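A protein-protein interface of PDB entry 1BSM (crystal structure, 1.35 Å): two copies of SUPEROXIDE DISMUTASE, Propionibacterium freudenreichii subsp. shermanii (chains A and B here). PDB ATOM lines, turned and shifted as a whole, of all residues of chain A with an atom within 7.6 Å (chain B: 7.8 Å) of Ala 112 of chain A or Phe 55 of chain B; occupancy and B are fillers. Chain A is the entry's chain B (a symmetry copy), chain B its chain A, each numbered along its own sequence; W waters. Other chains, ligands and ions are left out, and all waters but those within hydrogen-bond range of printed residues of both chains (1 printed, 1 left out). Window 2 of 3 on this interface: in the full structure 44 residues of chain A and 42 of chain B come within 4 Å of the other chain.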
ATOM      1  N   SER A 106       5.597  -4.472  23.839  1.00  0.00           N
ATOM      2  CA  SER A 106       4.944  -3.815  22.714  1.00  0.00           C
ATOM      3  C   SER A 106       5.453  -4.356  21.381  1.00  0.00           C
ATOM      4  O   SER A 106       6.368  -5.182  21.338  1.00  0.00           O
ATOM      5  CB  SER A 106       5.193  -2.305  22.774  1.00  0.00           C
ATOM      6  OG  SER A 106       6.558  -2.007  22.538  1.00  0.00           O
ATOM      7  N   PHE A 107       4.845  -3.880  20.298  1.00  0.00           N
ATOM      8  CA  PHE A 107       5.228  -4.275  18.947  1.00  0.00           C
ATOM      9  C   PHE A 107       6.613  -3.720  18.626  1.00  0.00           C
ATOM     10  O   PHE A 107       7.447  -4.410  18.036  1.00  0.00           O
ATOM     11  CB  PHE A 107       4.206  -3.742  17.938  1.00  0.00           C
ATOM     12  CG  PHE A 107       4.521  -4.086  16.508  1.00  0.00           C
ATOM     13  CD1 PHE A 107       4.704  -5.406  16.117  1.00  0.00           C
ATOM     14  CD2 PHE A 107       4.623  -3.085  15.546  1.00  0.00           C
ATOM     15  CE1 PHE A 107       4.985  -5.725  14.788  1.00  0.00           C
ATOM     16  CE2 PHE A 107       4.902  -3.395  14.214  1.00  0.00           C
ATOM     17  CZ  PHE A 107       5.082  -4.717  13.835  1.00  0.00           C
ATOM     18  N   ASP A 108       6.850  -2.469  19.018  1.00  0.00           N
ATOM     19  CA  ASP A 108       8.136  -1.823  18.776  1.00  0.00           C
ATOM     20  C   ASP A 108       9.272  -2.513  19.521  1.00  0.00           C
ATOM     21  O   ASP A 108      10.364  -2.672  18.976  1.00  0.00           O
ATOM     22  CB  ASP A 108       8.082  -0.338  19.149  1.00  0.00           C
ATOM     23  CG  ASP A 108       7.255   0.478  18.171  1.00  0.00           C
ATOM     24  OD1 ASP A 108       7.375   0.253  16.948  1.00  0.00           O
ATOM     25  OD2 ASP A 108       6.484   1.350  18.626  1.00  0.00           O
ATOM     26  N   ASN A 109       9.019  -2.909  20.767  1.00  0.00           N
ATOM     27  CA  ASN A 109      10.031  -3.601  21.561  1.00  0.00           C
ATOM     28  C   ASN A 109      10.366  -4.955  20.937  1.00  0.00           C
ATOM     29  O   ASN A 109      11.519  -5.384  20.952  1.00  0.00           O
ATOM     30  CB  ASN A 109       9.560  -3.782  23.006  1.00  0.00           C
ATOM     31  CG  ASN A 109       9.710  -2.516  23.834  1.00  0.00           C
ATOM     32  OD1 ASN A 109      10.237  -1.509  23.363  1.00  0.00           O
ATOM     33  ND2 ASN A 109       9.258  -2.570  25.083  1.00  0.00           N
ATOM     34  N   MET A 110       9.354  -5.613  20.375  1.00  0.00           N
ATOM     35  CA  MET A 110       9.546  -6.905  19.726  1.00  0.00           C
ATOM     36  C   MET A 110      10.426  -6.716  18.497  1.00  0.00           C
ATOM     37  O   MET A 110      11.353  -7.489  18.265  1.00  0.00           O
ATOM     38  CB  MET A 110       8.196  -7.505  19.326  1.00  0.00           C
ATOM     39  CG  MET A 110       8.270  -8.877  18.660  1.00  0.00           C
ATOM     40  SD  MET A 110       8.808  -8.832  16.940  1.00  0.00           S
ATOM     41  CE  MET A 110       7.362  -8.124  16.163  1.00  0.00           C
ATOM     42  N   LYS A 111      10.144  -5.666  17.730  1.00  0.00           N
ATOM     43  CA  LYS A 111      10.918  -5.365  16.531  1.00  0.00           C
ATOM     44  C   LYS A 111      12.362  -5.035  16.874  1.00  0.00           C
ATOM     45  O   LYS A 111      13.271  -5.471  16.184  1.00  0.00           O
ATOM     46  CB  LYS A 111      10.290  -4.204  15.760  1.00  0.00           C
ATOM     47  CG  LYS A 111       8.986  -4.562  15.074  1.00  0.00           C
ATOM     48  CD  LYS A 111       8.259  -3.328  14.579  1.00  0.00           C
ATOM     49  CE  LYS A 111       9.084  -2.539  13.590  1.00  0.00           C
ATOM     50  NZ  LYS A 111       8.304  -1.384  13.072  1.00  0.00           N
ATOM     51  N   ALA A 112      12.563  -4.272  17.945  1.00  0.00           N
ATOM     52  CA  ALA A 112      13.902  -3.889  18.384  1.00  0.00           C
ATOM     53  C   ALA A 112      14.753  -5.114  18.730  1.00  0.00           C
ATOM     54  O   ALA A 112      15.901  -5.214  18.304  1.00  0.00           O
ATOM     55  CB  ALA A 112      13.815  -2.949  19.579  1.00  0.00           C
ATOM     56  N   GLN A 113      14.181  -6.049  19.484  1.00  0.00           N
ATOM     57  CA  GLN A 113      14.896  -7.262  19.874  1.00  0.00           C
ATOM     58  C   GLN A 113      15.163  -8.156  18.662  1.00  0.00           C
ATOM     59  O   GLN A 113      16.255  -8.703  18.510  1.00  0.00           O
ATOM     60  CB  GLN A 113      14.100  -8.031  20.935  1.00  0.00           C
ATOM     61  CG  GLN A 113      14.816  -9.263  21.477  1.00  0.00           C
ATOM     62  CD  GLN A 113      14.128  -9.863  22.691  1.00  0.00           C
ATOM     63  OE1 GLN A 113      13.846 -11.064  22.729  1.00  0.00           O
ATOM     64  NE2 GLN A 113      13.878  -9.035  23.702  1.00  0.00           N
ATOM     65  N   PHE A 114      14.159  -8.276  17.796  1.00  0.00           N
ATOM     66  CA  PHE A 114      14.245  -9.089  16.585  1.00  0.00           C
ATOM     67  C   PHE A 114      15.302  -8.538  15.620  1.00  0.00           C
ATOM     68  O   PHE A 114      16.086  -9.301  15.049  1.00  0.00           O
ATOM     69  CB  PHE A 114      12.867  -9.131  15.907  1.00  0.00           C
ATOM     70  CG  PHE A 114      12.767 -10.103  14.761  1.00  0.00           C
ATOM     71  CD1 PHE A 114      13.259  -9.775  13.503  1.00  0.00           C
ATOM     72  CD2 PHE A 114      12.129 -11.329  14.928  1.00  0.00           C
ATOM     73  CE1 PHE A 114      13.116 -10.647  12.429  1.00  0.00           C
ATOM     74  CE2 PHE A 114      11.981 -12.208  13.856  1.00  0.00           C
ATOM     75  CZ  PHE A 114      12.476 -11.865  12.606  1.00  0.00           C
ATOM     76  N   THR A 115      15.328  -7.217  15.459  1.00  0.00           N
ATOM     77  CA  THR A 115      16.285  -6.570  14.562  1.00  0.00           C
ATOM     78  C   THR A 115      17.712  -6.749  15.056  1.00  0.00           C
ATOM     79  O   THR A 115      18.607  -7.053  14.273  1.00  0.00           O
ATOM     80  CB  THR A 115      16.005  -5.059  14.401  1.00  0.00           C
ATOM     81  OG1 THR A 115      16.038  -4.421  15.681  1.00  0.00           O
ATOM     82  CG2 THR A 115      14.654  -4.833  13.773  1.00  0.00           C
ATOM     83  N   ALA A 116      17.911  -6.553  16.358  1.00  0.00           N
ATOM     84  CA  ALA A 116      19.225  -6.703  16.974  1.00  0.00           C
ATOM     85  C   ALA A 116      19.752  -8.117  16.755  1.00  0.00           C
ATOM     86  O   ALA A 116      20.927  -8.313  16.446  1.00  0.00           O
ATOM     87  CB  ALA A 116      19.145  -6.388  18.454  1.00  0.00           C
ATOM     88  N   ALA A 117      18.866  -9.099  16.895  1.00  0.00           N
ATOM     89  CA  ALA A 117      19.232 -10.495  16.696  1.00  0.00           C
ATOM     90  C   ALA A 117      19.571 -10.741  15.227  1.00  0.00           C
ATOM     91  O   ALA A 117      20.481 -11.501  14.908  1.00  0.00           O
ATOM     92  CB  ALA A 117      18.087 -11.402  17.132  1.00  0.00           C
ATOM     93  N   ALA A 118      18.851 -10.061  14.339  1.00  0.00           N
ATOM     94  CA  ALA A 118      19.055 -10.208  12.901  1.00  0.00           C
ATOM     95  C   ALA A 118      20.376  -9.654  12.365  1.00  0.00           C
ATOM     96  O   ALA A 118      21.053 -10.314  11.577  1.00  0.00           O
ATOM     97  CB  ALA A 118      17.882  -9.588  12.145  1.00  0.00           C
ATOM     98  N   THR A 119      20.754  -8.457  12.808  1.00  0.00           N
ATOM     99  CA  THR A 119      21.980  -7.822  12.324  1.00  0.00           C
ATOM    100  C   THR A 119      23.268  -8.191  13.052  1.00  0.00           C
ATOM    101  O   THR A 119      24.359  -7.915  12.556  1.00  0.00           O
ATOM    102  CB  THR A 119      21.853  -6.285  12.319  1.00  0.00           C
ATOM    103  OG1 THR A 119      21.720  -5.806  13.661  1.00  0.00           O
ATOM    104  CG2 THR A 119      20.638  -5.855  11.517  1.00  0.00           C
ATOM    105  N   GLY A 120      23.145  -8.823  14.216  1.00  0.00           N
ATOM    106  CA  GLY A 120      24.328  -9.188  14.978  1.00  0.00           C
ATOM    107  C   GLY A 120      24.945 -10.551  14.727  1.00  0.00           C
ATOM    108  O   GLY A 120      26.022 -10.835  15.249  1.00  0.00           O
ATOM    109  N   THR A 140      12.325 -14.804  20.815  1.00  0.00           N
ATOM    110  CA  THR A 140      13.063 -14.543  19.588  1.00  0.00           C
ATOM    111  C   THR A 140      14.300 -15.425  19.703  1.00  0.00           C
ATOM    112  O   THR A 140      14.833 -15.619  20.801  1.00  0.00           O
ATOM    113  CB  THR A 140      13.520 -13.069  19.422  1.00  0.00           C
ATOM    114  OG1 THR A 140      14.353 -12.686  20.521  1.00  0.00           O
ATOM    115  CG2 THR A 140      12.328 -12.132  19.310  1.00  0.00           C
ATOM    116  N   TRP A 183      10.475  -5.349   7.146  1.00  0.00           N
ATOM    117  CA  TRP A 183       9.293  -5.206   8.000  1.00  0.00           C
ATOM    118  C   TRP A 183       8.073  -4.738   7.209  1.00  0.00           C
ATOM    119  O   TRP A 183       6.939  -5.077   7.549  1.00  0.00           O
ATOM    120  CB  TRP A 183       9.552  -4.227   9.147  1.00  0.00           C
ATOM    121  CG  TRP A 183      10.438  -4.763  10.227  1.00  0.00           C
ATOM    122  CD1 TRP A 183      11.693  -4.335  10.540  1.00  0.00           C
ATOM    123  CD2 TRP A 183      10.126  -5.811  11.155  1.00  0.00           C
ATOM    124  NE1 TRP A 183      12.182  -5.050  11.606  1.00  0.00           N
ATOM    125  CE2 TRP A 183      11.245  -5.963  12.007  1.00  0.00           C
ATOM    126  CE3 TRP A 183       9.008  -6.637  11.355  1.00  0.00           C
ATOM    127  CZ2 TRP A 183      11.281  -6.907  13.039  1.00  0.00           C
ATOM    128  CZ3 TRP A 183       9.046  -7.578  12.384  1.00  0.00           C
ATOM    129  CH2 TRP A 183      10.176  -7.704  13.211  1.00  0.00           C
ATOM    130  N   LYS B  45      17.427 -10.995  31.215  1.00  0.00           N
ATOM    131  CA  LYS B  45      18.392 -10.130  30.545  1.00  0.00           C
ATOM    132  C   LYS B  45      17.838  -9.550  29.250  1.00  0.00           C
ATOM    133  O   LYS B  45      18.132  -8.406  28.904  1.00  0.00           O
ATOM    134  CB  LYS B  45      19.687 -10.892  30.265  1.00  0.00           C
ATOM    135  CG  LYS B  45      20.832 -10.533  31.196  1.00  0.00           C
ATOM    136  CD  LYS B  45      20.482 -10.794  32.649  1.00  0.00           C
ATOM    137  CE  LYS B  45      21.597 -10.337  33.579  1.00  0.00           C
ATOM    138  NZ  LYS B  45      21.862  -8.875  33.466  1.00  0.00           N
ATOM    139  N   LEU B  46      17.057 -10.348  28.530  1.00  0.00           N
ATOM    140  CA  LEU B  46      16.448  -9.896  27.284  1.00  0.00           C
ATOM    141  C   LEU B  46      15.411  -8.810  27.575  1.00  0.00           C
ATOM    142  O   LEU B  46      15.326  -7.817  26.853  1.00  0.00           O
ATOM    143  CB  LEU B  46      15.816 -11.075  26.543  1.00  0.00           C
ATOM    144  CG  LEU B  46      16.816 -11.983  25.820  1.00  0.00           C
ATOM    145  CD1 LEU B  46      16.171 -13.302  25.439  1.00  0.00           C
ATOM    146  CD2 LEU B  46      17.366 -11.273  24.589  1.00  0.00           C
ATOM    147  N   ALA B  47      14.647  -8.992  28.652  1.00  0.00           N
ATOM    148  CA  ALA B  47      13.640  -8.013  29.060  1.00  0.00           C
ATOM    149  C   ALA B  47      14.345  -6.713  29.440  1.00  0.00           C
ATOM    150  O   ALA B  47      13.901  -5.622  29.083  1.00  0.00           O
ATOM    151  CB  ALA B  47      12.834  -8.544  30.241  1.00  0.00           C
ATOM    152  N   GLU B  48      15.452  -6.849  30.167  1.00  0.00           N
ATOM    153  CA  GLU B  48      16.258  -5.712  30.594  1.00  0.00           C
ATOM    154  C   GLU B  48      16.796  -4.981  29.364  1.00  0.00           C
ATOM    155  O   GLU B  48      16.856  -3.751  29.342  1.00  0.00           O
ATOM    156  CB  GLU B  48      17.418  -6.205  31.462  1.00  0.00           C
ATOM    157  CG  GLU B  48      18.360  -5.119  31.945  1.00  0.00           C
ATOM    158  CD  GLU B  48      19.522  -5.674  32.750  1.00  0.00           C
ATOM    159  OE1 GLU B  48      20.508  -6.134  32.137  1.00  0.00           O
ATOM    160  OE2 GLU B  48      19.452  -5.649  33.997  1.00  0.00           O
ATOM    161  N   ALA B  49      17.186  -5.754  28.350  1.00  0.00           N
ATOM    162  CA  ALA B  49      17.710  -5.211  27.099  1.00  0.00           C
ATOM    163  C   ALA B  49      16.653  -4.371  26.383  1.00  0.00           C
ATOM    164  O   ALA B  49      16.962  -3.319  25.818  1.00  0.00           O
ATOM    165  CB  ALA B  49      18.188  -6.339  26.196  1.00  0.00           C
ATOM    166  N   ARG B  50      15.410  -4.841  26.411  1.00  0.00           N
ATOM    167  CA  ARG B  50      14.308  -4.124  25.780  1.00  0.00           C
ATOM    168  C   ARG B  50      13.984  -2.843  26.543  1.00  0.00           C
ATOM    169  O   ARG B  50      13.692  -1.810  25.937  1.00  0.00           O
ATOM    170  CB  ARG B  50      13.064  -5.013  25.689  1.00  0.00           C
ATOM    171  CG  ARG B  50      13.230  -6.221  24.776  1.00  0.00           C
ATOM    172  CD  ARG B  50      11.902  -6.922  24.515  1.00  0.00           C
ATOM    173  NE  ARG B  50      11.271  -7.408  25.740  1.00  0.00           N
ATOM    174  CZ  ARG B  50      11.471  -8.614  26.264  1.00  0.00           C
ATOM    175  NH1 ARG B  50      12.291  -9.477  25.677  1.00  0.00           N
ATOM    176  NH2 ARG B  50      10.844  -8.963  27.380  1.00  0.00           N
ATOM    177  N   ASP B  51      14.064  -2.909  27.872  1.00  0.00           N
ATOM    178  CA  ASP B  51      13.785  -1.757  28.729  1.00  0.00           C
ATOM    179  C   ASP B  51      14.735  -0.589  28.476  1.00  0.00           C
ATOM    180  O   ASP B  51      14.301   0.553  28.342  1.00  0.00           O
ATOM    181  CB  ASP B  51      13.874  -2.141  30.212  1.00  0.00           C
ATOM    182  CG  ASP B  51      12.750  -3.059  30.661  1.00  0.00           C
ATOM    183  OD1 ASP B  51      11.673  -3.071  30.025  1.00  0.00           O
ATOM    184  OD2 ASP B  51      12.946  -3.768  31.670  1.00  0.00           O
ATOM    185  N   LYS B  52      16.033  -0.885  28.424  1.00  0.00           N
ATOM    186  CA  LYS B  52      17.055   0.141  28.218  1.00  0.00           C
ATOM    187  C   LYS B  52      17.426   0.353  26.753  1.00  0.00           C
ATOM    188  O   LYS B  52      18.228   1.238  26.439  1.00  0.00           O
ATOM    189  CB  LYS B  52      18.329  -0.224  28.983  1.00  0.00           C
ATOM    190  CG  LYS B  52      18.133  -0.627  30.430  1.00  0.00           C
ATOM    191  CD  LYS B  52      19.412  -1.244  30.960  1.00  0.00           C
ATOM    192  CE  LYS B  52      19.297  -1.610  32.425  1.00  0.00           C
ATOM    193  NZ  LYS B  52      20.519  -2.325  32.888  1.00  0.00           N
ATOM    194  N   ALA B  53      16.873  -0.472  25.869  1.00  0.00           N
ATOM    195  CA  ALA B  53      17.162  -0.390  24.436  1.00  0.00           C
ATOM    196  C   ALA B  53      18.649  -0.654  24.193  1.00  0.00           C
ATOM    197  O   ALA B  53      19.284  -0.004  23.360  1.00  0.00           O
ATOM    198  CB  ALA B  53      16.756   0.978  23.879  1.00  0.00           C
ATOM    199  N   ASP B  54      19.199  -1.592  24.960  1.00  0.00           N
ATOM    200  CA  ASP B  54      20.606  -1.967  24.858  1.00  0.00           C
ATOM    201  C   ASP B  54      20.715  -3.461  24.553  1.00  0.00           C
ATOM    202  O   ASP B  54      20.674  -4.299  25.455  1.00  0.00           O
ATOM    203  CB  ASP B  54      21.338  -1.624  26.168  1.00  0.00           C
ATOM    204  CG  ASP B  54      22.830  -1.960  26.135  1.00  0.00           C
ATOM    205  OD1 ASP B  54      23.338  -2.470  25.114  1.00  0.00           O
ATOM    206  OD2 ASP B  54      23.504  -1.707  27.153  1.00  0.00           O
ATOM    207  N   PHE B  55      20.859  -3.777  23.269  1.00  0.00           N
ATOM    208  CA  PHE B  55      20.980  -5.157  22.817  1.00  0.00           C
ATOM    209  C   PHE B  55      22.428  -5.487  22.444  1.00  0.00           C
ATOM    210  O   PHE B  55      22.676  -6.316  21.568  1.00  0.00           O
ATOM    211  CB  PHE B  55      20.060  -5.409  21.611  1.00  0.00           C
ATOM    212  CG  PHE B  55      18.608  -5.097  21.868  1.00  0.00           C
ATOM    213  CD1 PHE B  55      17.764  -6.062  22.409  1.00  0.00           C
ATOM    214  CD2 PHE B  55      18.084  -3.841  21.571  1.00  0.00           C
ATOM    215  CE1 PHE B  55      16.418  -5.784  22.650  1.00  0.00           C
ATOM    216  CE2 PHE B  55      16.737  -3.548  21.808  1.00  0.00           C
ATOM    217  CZ  PHE B  55      15.902  -4.525  22.347  1.00  0.00           C
ATOM    218  N   GLY B  56      23.379  -4.856  23.132  1.00  0.00           N
ATOM    219  CA  GLY B  56      24.788  -5.094  22.858  1.00  0.00           C
ATOM    220  C   GLY B  56      25.210  -6.546  23.002  1.00  0.00           C
ATOM    221  O   GLY B  56      26.059  -7.028  22.251  1.00  0.00           O
ATOM    222  N   ALA B  57      24.601  -7.247  23.957  1.00  0.00           N
ATOM    223  CA  ALA B  57      24.908  -8.652  24.206  1.00  0.00           C
ATOM    224  C   ALA B  57      23.854  -9.595  23.628  1.00  0.00           C
ATOM    225  O   ALA B  57      23.695 -10.713  24.112  1.00  0.00           O
ATOM    226  CB  ALA B  57      25.053  -8.889  25.702  1.00  0.00           C
ATOM    227  N   ILE B  58      23.164  -9.160  22.576  1.00  0.00           N
ATOM    228  CA  ILE B  58      22.119  -9.976  21.963  1.00  0.00           C
ATOM    229  C   ILE B  58      22.595 -11.356  21.506  1.00  0.00           C
ATOM    230  O   ILE B  58      21.879 -12.341  21.675  1.00  0.00           O
ATOM    231  CB  ILE B  58      21.411  -9.231  20.798  1.00  0.00           C
ATOM    232  CG1 ILE B  58      20.193 -10.028  20.317  1.00  0.00           C
ATOM    233  CG2 ILE B  58      22.378  -8.977  19.646  1.00  0.00           C
ATOM    234  CD1 ILE B  58      19.102 -10.187  21.365  1.00  0.00           C
ATOM    235  N   ASN B  59      23.804 -11.433  20.955  1.00  0.00           N
ATOM    236  CA  ASN B  59      24.342 -12.710  20.493  1.00  0.00           C
ATOM    237  C   ASN B  59      24.525 -13.667  21.671  1.00  0.00           C
ATOM    238  O   ASN B  59      24.223 -14.858  21.567  1.00  0.00           O
ATOM    239  CB  ASN B  59      25.676 -12.510  19.764  1.00  0.00           C
ATOM    240  CG  ASN B  59      25.530 -11.711  18.481  1.00  0.00           C
ATOM    241  OD1 ASN B  59      24.430 -11.569  17.944  1.00  0.00           O
ATOM    242  ND2 ASN B  59      26.643 -11.176  17.985  1.00  0.00           N
ATOM    243  N   LYS B  60      25.002 -13.129  22.792  1.00  0.00           N
ATOM    244  CA  LYS B  60      25.215 -13.905  24.007  1.00  0.00           C
ATOM    245  C   LYS B  60      23.889 -14.397  24.581  1.00  0.00           C
ATOM    246  O   LYS B  60      23.738 -15.577  24.893  1.00  0.00           O
ATOM    247  CB  LYS B  60      25.929 -13.048  25.060  1.00  0.00           C
ATOM    248  CG  LYS B  60      25.923 -13.649  26.460  1.00  0.00           C
ATOM    249  CD  LYS B  60      26.445 -12.670  27.496  1.00  0.00           C
ATOM    250  CE  LYS B  60      26.199 -13.171  28.913  1.00  0.00           C
ATOM    251  NZ  LYS B  60      26.818 -14.504  29.160  1.00  0.00           N
ATOM    252  N   LEU B  61      22.937 -13.480  24.720  1.00  0.00           N
ATOM    253  CA  LEU B  61      21.629 -13.800  25.277  1.00  0.00           C
ATOM    254  C   LEU B  61      20.829 -14.798  24.446  1.00  0.00           C
ATOM    255  O   LEU B  61      20.134 -15.647  24.999  1.00  0.00           O
ATOM    256  CB  LEU B  61      20.824 -12.519  25.504  1.00  0.00           C
ATOM    257  CG  LEU B  61      21.492 -11.501  26.432  1.00  0.00           C
ATOM    258  CD1 LEU B  61      20.598 -10.285  26.608  1.00  0.00           C
ATOM    259  CD2 LEU B  61      21.808 -12.144  27.775  1.00  0.00           C
HETATM  260  O   HOH W   1      12.511 -12.534  25.127  1.00  0.00           O
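Of the 17 printed residues of chain B, 5 touch a printed residue of chain A. Hydrophobic or aromatic side chains of chain B that line the printed part of chain A: Leu 46, Phe 55 and Ile 58. Along chain B the printed residues that touch a printed residue of chain A span positions 46 to 59.
No position is printed for both chains. Of the 9 pairs that touch across the chains among the printed residues, none has its exchanged pair printed and touching as well.
Ala 112 of chain A touches one residue of chain B. Printed residues of chain B within 4 Å of Gln 113 of chain A: Leu 46 (3.7 Å), Arg 50 (2.6 Å) and Phe 55 (3.5 Å). Printed residues of chain B within 4 Å of Gly 120 of chain A: Asn 59 (2.8 Å). Ala 47 of chain B touches none of the printed residues of chain A. Printed residues of chain A within 4 Å of Arg 50 of chain B: Asn 109 and Gln 113. Of chain A, only Ala 112 (3.7 Å), Gln 113 (3.5 Å) and Ala 116 (3.4 Å) come within 4 Å of Phe 55 of chain B. No residue of chain A comes within 4 Å of Gly 56 of chain B. Of the printed residues of chain A, Ile 58 of chain B touches Ala 116 and Ala 117. Of the printed residues of chain A, Asn 59 of chain B touches Gly 120 (2.8 Å). The nearest residue of chain B that does not touch Ala 112 of chain A is Arg 50 of chain B (6.2 Å).
OG of Ser 106 of chain A sits at hydrogen-bond distance from N of Asn 109 of chain A, at 3.2 Å. The side-chain hydroxyl of Thr 115 of chain A sits at hydrogen-bond distance from the backbone carbonyl oxygen of Ala 112 of chain A, 2.7 Å away. OE1 of Gln 113 of chain A is in hydrogen-bond range of OG1 of Thr 140 of chain A (2.8 Å).
Among the printed residues, pairs that only touch across the chains: Ala 116 of chain A with Phe 55 of chain B (3.4 Å), Gln 113 of chain A with Phe 55 of chain B (3.5 Å), Ala 116 of chain A with Ile 58 of chain B (3.6 Å), Gln 113 of chain A with Leu 46 of chain B (3.7 Å), Ala 112 of chain A with Phe 55 of chain B (3.7 Å), Ala 117 of chain A with Ile 58 of chain B (3.8 Å) and Asn 109 of chain A with Arg 50 of chain B (3.9 Å).
Water W1 bridges the side-chain amide oxygen of Gln 113 of chain A (3.1 Å) and the guanidinium group of Arg 50 of chain B (3.1 Å).
The side-chain amide nitrogen (ND2) of Asn 59 of chain B lies within hydrogen-bond range of the backbone carbonyl oxygen (O) of Gly 120 of chain A (2.8 Å). NE2 of Gln 113 of chain A lies close to NH1 of Arg 50 of chain B (2.6 Å).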
